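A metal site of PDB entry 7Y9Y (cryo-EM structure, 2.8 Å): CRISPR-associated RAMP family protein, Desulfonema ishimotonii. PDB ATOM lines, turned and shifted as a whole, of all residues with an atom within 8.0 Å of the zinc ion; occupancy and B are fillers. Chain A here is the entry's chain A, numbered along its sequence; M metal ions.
The side-chain sulfur of Cys 123 sits close to the backbone NH of Phe 125, 3.5 Å away. The backbone NH of Arg 131 is in hydrogen-bond range of the backbone carbonyl oxygen of Cys 126 (3.0 Å). The indole nitrogen (NE1) of Trp 109 sits at hydrogen-bond distance from the backbone carbonyl oxygen (O) of Cys 86, 3.4 Å away. The guanidinium group (NH2) of Arg 131 is in hydrogen-bond range of the backbone carbonyl oxygen (O) of Cys 115, 3.3 Å away. The side-chain sulfur of Cys 86 lies close to the backbone NH of Gly 88, 3.3 Å away.
Of the 22 residues printed, 4 come within 4 Å of the zinc ion. The nearest printed residue that does not touch the zinc ion is Arg 131 (4.6 Å).
The zinc ion is bound by the side-chain sulfur (SG) of Cys 86 (2.3 Å), the side-chain sulfur (SG) of Cys 126 (2.3 Å), the side-chain sulfur (SG) of Cys 115 (2.3 Å) and the side-chain sulfur (SG) of Cys 123 (2.3 Å).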
ATOM      1  N   LYS A  83      12.624  -1.419  30.640  1.00  0.00           N
ATOM      2  CA  LYS A  83      13.331  -0.152  30.733  1.00  0.00           C
ATOM      3  C   LYS A  83      12.540   0.861  31.565  1.00  0.00           C
ATOM      4  O   LYS A  83      11.319   0.810  31.672  1.00  0.00           O
ATOM      5  CB  LYS A  83      13.592   0.419  29.337  1.00  0.00           C
ATOM      6  CG  LYS A  83      14.661  -0.330  28.559  1.00  0.00           C
ATOM      7  CD  LYS A  83      15.257   0.551  27.477  1.00  0.00           C
ATOM      8  CE  LYS A  83      16.010   1.730  28.076  1.00  0.00           C
ATOM      9  NZ  LYS A  83      16.645   2.579  27.030  1.00  0.00           N
ATOM     10  N   THR A  84      13.281   1.792  32.165  1.00  0.00           N
ATOM     11  CA  THR A  84      12.721   2.914  32.915  1.00  0.00           C
ATOM     12  C   THR A  84      12.939   4.202  32.127  1.00  0.00           C
ATOM     13  O   THR A  84      13.804   4.272  31.252  1.00  0.00           O
ATOM     14  CB  THR A  84      13.373   3.015  34.303  1.00  0.00           C
ATOM     15  OG1 THR A  84      13.665   1.700  34.790  1.00  0.00           O
ATOM     16  CG2 THR A  84      12.431   3.702  35.283  1.00  0.00           C
ATOM     17  N   CYS A  85      12.142   5.209  32.456  1.00  0.00           N
ATOM     18  CA  CYS A  85      12.153   6.468  31.714  1.00  0.00           C
ATOM     19  C   CYS A  85      12.500   7.624  32.630  1.00  0.00           C
ATOM     20  O   CYS A  85      12.032   7.684  33.778  1.00  0.00           O
ATOM     21  CB  CYS A  85      10.793   6.732  31.048  1.00  0.00           C
ATOM     22  SG  CYS A  85      10.328   5.521  29.795  1.00  0.00           S
ATOM     23  N   CYS A  86      13.320   8.550  32.123  1.00  0.00           N
ATOM     24  CA  CYS A  86      13.606   9.782  32.824  1.00  0.00           C
ATOM     25  C   CYS A  86      12.424  10.733  32.691  1.00  0.00           C
ATOM     26  O   CYS A  86      11.520  10.511  31.875  1.00  0.00           O
ATOM     27  CB  CYS A  86      14.867  10.431  32.261  1.00  0.00           C
ATOM     28  SG  CYS A  86      14.635  11.254  30.671  1.00  0.00           S
ATOM     29  N   PRO A  87      12.384  11.811  33.489  1.00  0.00           N
ATOM     30  CA  PRO A  87      11.266  12.764  33.377  1.00  0.00           C
ATOM     31  C   PRO A  87      11.187  13.488  32.042  1.00  0.00           C
ATOM     32  O   PRO A  87      10.179  14.157  31.785  1.00  0.00           O
ATOM     33  CB  PRO A  87      11.598  13.691  34.529  1.00  0.00           C
ATOM     34  CG  PRO A  87      13.066  13.709  34.214  1.00  0.00           C
ATOM     35  CD  PRO A  87      13.216  12.312  34.595  1.00  0.00           C
ATOM     36  N   GLY A  88      12.203  13.386  31.195  1.00  0.00           N
ATOM     37  CA  GLY A  88      12.225  14.102  29.937  1.00  0.00           C
ATOM     38  C   GLY A  88      12.703  15.537  30.088  1.00  0.00           C
ATOM     39  O   GLY A  88      12.860  16.062  31.195  1.00  0.00           O
ATOM     40  N   LYS A  89      12.927  16.185  28.945  1.00  0.00           N
ATOM     41  CA  LYS A  89      13.433  17.542  28.919  1.00  0.00           C
ATOM     42  C   LYS A  89      12.423  18.442  28.223  1.00  0.00           C
ATOM     43  O   LYS A  89      12.000  18.151  27.099  1.00  0.00           O
ATOM     44  CB  LYS A  89      14.788  17.628  28.215  1.00  0.00           C
ATOM     45  CG  LYS A  89      15.251  19.045  27.930  1.00  0.00           C
ATOM     46  CD  LYS A  89      16.729  19.082  27.593  1.00  0.00           C
ATOM     47  CE  LYS A  89      17.584  18.814  28.819  1.00  0.00           C
ATOM     48  NZ  LYS A  89      19.032  19.134  28.579  1.00  0.00           N
ATOM     49  N   TRP A 109       7.112  11.143  37.483  1.00  0.00           N
ATOM     50  CA  TRP A 109       7.087   9.774  37.986  1.00  0.00           C
ATOM     51  C   TRP A 109       8.359   9.433  38.756  1.00  0.00           C
ATOM     52  O   TRP A 109       8.302   8.878  39.845  1.00  0.00           O
ATOM     53  CB  TRP A 109       6.877   8.769  36.841  1.00  0.00           C
ATOM     54  CG  TRP A 109       7.618   9.088  35.577  1.00  0.00           C
ATOM     55  CD1 TRP A 109       8.857   8.640  35.233  1.00  0.00           C
ATOM     56  CD2 TRP A 109       7.163   9.869  34.471  1.00  0.00           C
ATOM     57  NE1 TRP A 109       9.214   9.111  33.995  1.00  0.00           N
ATOM     58  CE2 TRP A 109       8.179   9.876  33.503  1.00  0.00           C
ATOM     59  CE3 TRP A 109       5.988  10.583  34.211  1.00  0.00           C
ATOM     60  CZ2 TRP A 109       8.068  10.561  32.294  1.00  0.00           C
ATOM     61  CZ3 TRP A 109       5.876  11.257  33.015  1.00  0.00           C
ATOM     62  CH2 TRP A 109       6.907  11.244  32.070  1.00  0.00           C
ATOM     63  N   LYS A 112      15.167  11.003  38.986  1.00  0.00           N
ATOM     64  CA  LYS A 112      16.520  11.142  38.476  1.00  0.00           C
ATOM     65  C   LYS A 112      16.552  12.174  37.362  1.00  0.00           C
ATOM     66  O   LYS A 112      15.532  12.551  36.796  1.00  0.00           O
ATOM     67  CB  LYS A 112      17.097   9.808  37.965  1.00  0.00           C
ATOM     68  CG  LYS A 112      16.687   9.387  36.561  1.00  0.00           C
ATOM     69  CD  LYS A 112      16.188   7.954  36.512  1.00  0.00           C
ATOM     70  CE  LYS A 112      14.748   7.852  36.902  1.00  0.00           C
ATOM     71  NZ  LYS A 112      14.227   6.465  36.822  1.00  0.00           N
ATOM     72  N   ASN A 113      17.759  12.653  37.062  1.00  0.00           N
ATOM     73  CA  ASN A 113      17.940  13.697  36.069  1.00  0.00           C
ATOM     74  C   ASN A 113      17.618  13.180  34.671  1.00  0.00           C
ATOM     75  O   ASN A 113      17.661  11.975  34.418  1.00  0.00           O
ATOM     76  CB  ASN A 113      19.359  14.231  36.118  1.00  0.00           C
ATOM     77  CG  ASN A 113      19.520  15.382  37.087  1.00  0.00           C
ATOM     78  OD1 ASN A 113      18.561  16.101  37.382  1.00  0.00           O
ATOM     79  ND2 ASN A 113      20.735  15.571  37.591  1.00  0.00           N
ATOM     80  N   PRO A 114      17.279  14.073  33.741  1.00  0.00           N
ATOM     81  CA  PRO A 114      17.014  13.649  32.368  1.00  0.00           C
ATOM     82  C   PRO A 114      18.234  13.021  31.715  1.00  0.00           C
ATOM     83  O   PRO A 114      19.358  13.120  32.210  1.00  0.00           O
ATOM     84  CB  PRO A 114      16.614  14.951  31.669  1.00  0.00           C
ATOM     85  CG  PRO A 114      16.098  15.820  32.769  1.00  0.00           C
ATOM     86  CD  PRO A 114      16.963  15.494  33.953  1.00  0.00           C
ATOM     87  N   CYS A 115      17.990  12.372  30.585  1.00  0.00           N
ATOM     88  CA  CYS A 115      19.060  11.732  29.833  1.00  0.00           C
ATOM     89  C   CYS A 115      20.083  12.781  29.387  1.00  0.00           C
ATOM     90  O   CYS A 115      19.720  13.937  29.118  1.00  0.00           O
ATOM     91  CB  CYS A 115      18.505  10.990  28.615  1.00  0.00           C
ATOM     92  SG  CYS A 115      17.476   9.552  28.999  1.00  0.00           S
ATOM     93  N   PRO A 116      21.357  12.408  29.322  1.00  0.00           N
ATOM     94  CA  PRO A 116      22.385  13.375  28.903  1.00  0.00           C
ATOM     95  C   PRO A 116      22.106  13.908  27.509  1.00  0.00           C
ATOM     96  O   PRO A 116      21.574  13.208  26.647  1.00  0.00           O
ATOM     97  CB  PRO A 116      23.672  12.547  28.945  1.00  0.00           C
ATOM     98  CG  PRO A 116      23.397  11.459  29.931  1.00  0.00           C
ATOM     99  CD  PRO A 116      21.942  11.137  29.759  1.00  0.00           C
ATOM    100  N   THR A 121      22.814   5.816  24.601  1.00  0.00           N
ATOM    101  CA  THR A 121      21.533   5.186  24.854  1.00  0.00           C
ATOM    102  C   THR A 121      20.563   6.210  25.444  1.00  0.00           C
ATOM    103  O   THR A 121      20.913   6.958  26.352  1.00  0.00           O
ATOM    104  CB  THR A 121      21.670   4.009  25.819  1.00  0.00           C
ATOM    105  OG1 THR A 121      22.087   4.479  27.103  1.00  0.00           O
ATOM    106  CG2 THR A 121      22.707   3.015  25.292  1.00  0.00           C
ATOM    107  N   TYR A 122      19.340   6.226  24.913  1.00  0.00           N
ATOM    108  CA  TYR A 122      18.301   7.114  25.377  1.00  0.00           C
ATOM    109  C   TYR A 122      17.111   6.293  25.869  1.00  0.00           C
ATOM    110  O   TYR A 122      16.814   5.220  25.340  1.00  0.00           O
ATOM    111  CB  TYR A 122      17.832   8.067  24.268  1.00  0.00           C
ATOM    112  CG  TYR A 122      18.597   9.374  24.214  1.00  0.00           C
ATOM    113  CD1 TYR A 122      19.880   9.436  23.693  1.00  0.00           C
ATOM    114  CD2 TYR A 122      18.020  10.546  24.674  1.00  0.00           C
ATOM    115  CE1 TYR A 122      20.569  10.622  23.643  1.00  0.00           C
ATOM    116  CE2 TYR A 122      18.705  11.745  24.620  1.00  0.00           C
ATOM    117  CZ  TYR A 122      19.976  11.780  24.097  1.00  0.00           C
ATOM    118  OH  TYR A 122      20.665  12.966  24.047  1.00  0.00           O
ATOM    119  N   CYS A 123      16.438   6.809  26.891  1.00  0.00           N
ATOM    120  CA  CYS A 123      15.257   6.148  27.418  1.00  0.00           C
ATOM    121  C   CYS A 123      14.126   6.220  26.402  1.00  0.00           C
ATOM    122  O   CYS A 123      14.110   7.103  25.539  1.00  0.00           O
ATOM    123  CB  CYS A 123      14.844   6.788  28.747  1.00  0.00           C
ATOM    124  SG  CYS A 123      13.759   8.214  28.594  1.00  0.00           S
ATOM    125  N   PRO A 124      13.166   5.291  26.462  1.00  0.00           N
ATOM    126  CA  PRO A 124      12.094   5.268  25.458  1.00  0.00           C
ATOM    127  C   PRO A 124      11.293   6.557  25.396  1.00  0.00           C
ATOM    128  O   PRO A 124      10.824   6.925  24.307  1.00  0.00           O
ATOM    129  CB  PRO A 124      11.221   4.095  25.912  1.00  0.00           C
ATOM    130  CG  PRO A 124      12.164   3.192  26.631  1.00  0.00           C
ATOM    131  CD  PRO A 124      13.091   4.116  27.362  1.00  0.00           C
ATOM    132  N   PHE A 125      11.112   7.259  26.515  1.00  0.00           N
ATOM    133  CA  PHE A 125      10.370   8.507  26.490  1.00  0.00           C
ATOM    134  C   PHE A 125      11.097   9.563  25.674  1.00  0.00           C
ATOM    135  O   PHE A 125      10.477  10.391  25.010  1.00  0.00           O
ATOM    136  CB  PHE A 125      10.109   8.993  27.923  1.00  0.00           C
ATOM    137  CG  PHE A 125       9.287  10.238  28.006  1.00  0.00           C
ATOM    138  CD1 PHE A 125       7.917  10.190  27.774  1.00  0.00           C
ATOM    139  CD2 PHE A 125       9.857  11.440  28.358  1.00  0.00           C
ATOM    140  CE1 PHE A 125       7.147  11.333  27.855  1.00  0.00           C
ATOM    141  CE2 PHE A 125       9.082  12.585  28.448  1.00  0.00           C
ATOM    142  CZ  PHE A 125       7.734  12.529  28.194  1.00  0.00           C
ATOM    143  N   CYS A 126      12.436   9.539  25.709  1.00  0.00           N
ATOM    144  CA  CYS A 126      13.207  10.476  24.890  1.00  0.00           C
ATOM    145  C   CYS A 126      13.153  10.105  23.423  1.00  0.00           C
ATOM    146  O   CYS A 126      13.117  10.986  22.549  1.00  0.00           O
ATOM    147  CB  CYS A 126      14.650  10.527  25.386  1.00  0.00           C
ATOM    148  SG  CYS A 126      14.870  11.411  26.942  1.00  0.00           S
ATOM    149  N   GLU A 127      13.148   8.805  23.105  1.00  0.00           N
ATOM    150  CA  GLU A 127      12.987   8.389  21.716  1.00  0.00           C
ATOM    151  C   GLU A 127      11.635   8.818  21.174  1.00  0.00           C
ATOM    152  O   GLU A 127      11.530   9.254  20.022  1.00  0.00           O
ATOM    153  CB  GLU A 127      13.158   6.875  21.582  1.00  0.00           C
ATOM    154  CG  GLU A 127      14.398   6.312  22.260  1.00  0.00           C
ATOM    155  CD  GLU A 127      14.631   4.861  21.909  1.00  0.00           C
ATOM    156  OE1 GLU A 127      14.669   4.539  20.709  1.00  0.00           O
ATOM    157  OE2 GLU A 127      14.775   4.036  22.839  1.00  0.00           O
ATOM    158  N   LEU A 129      10.005  11.397  22.344  1.00  0.00           N
ATOM    159  CA  LEU A 129      10.149  12.839  22.231  1.00  0.00           C
ATOM    160  C   LEU A 129      10.892  13.224  20.956  1.00  0.00           C
ATOM    161  O   LEU A 129      10.535  14.205  20.298  1.00  0.00           O
ATOM    162  CB  LEU A 129      10.885  13.387  23.451  1.00  0.00           C
ATOM    163  CG  LEU A 129      10.090  13.677  24.721  1.00  0.00           C
ATOM    164  CD1 LEU A 129      11.041  14.022  25.858  1.00  0.00           C
ATOM    165  CD2 LEU A 129       9.120  14.813  24.495  1.00  0.00           C
ATOM    166  N   ARG A 131      14.580  13.137  21.086  1.00  0.00           N
ATOM    167  CA  ARG A 131      15.914  13.587  21.481  1.00  0.00           C
ATOM    168  C   ARG A 131      17.003  12.780  20.791  1.00  0.00           C
ATOM    169  O   ARG A 131      18.022  13.343  20.368  1.00  0.00           O
ATOM    170  CB  ARG A 131      16.066  13.502  22.996  1.00  0.00           C
ATOM    171  CG  ARG A 131      14.838  13.949  23.766  1.00  0.00           C
ATOM    172  CD  ARG A 131      15.075  15.268  24.496  1.00  0.00           C
ATOM    173  NE  ARG A 131      16.446  15.399  24.964  1.00  0.00           N
ATOM    174  CZ  ARG A 131      16.915  14.863  26.082  1.00  0.00           C
ATOM    175  NH1 ARG A 131      16.140  14.151  26.884  1.00  0.00           N
ATOM    176  NH2 ARG A 131      18.189  15.060  26.410  1.00  0.00           N
HETATM  177 ZN    ZN M   1      15.209  10.037  28.783  1.00  0.00          ZN
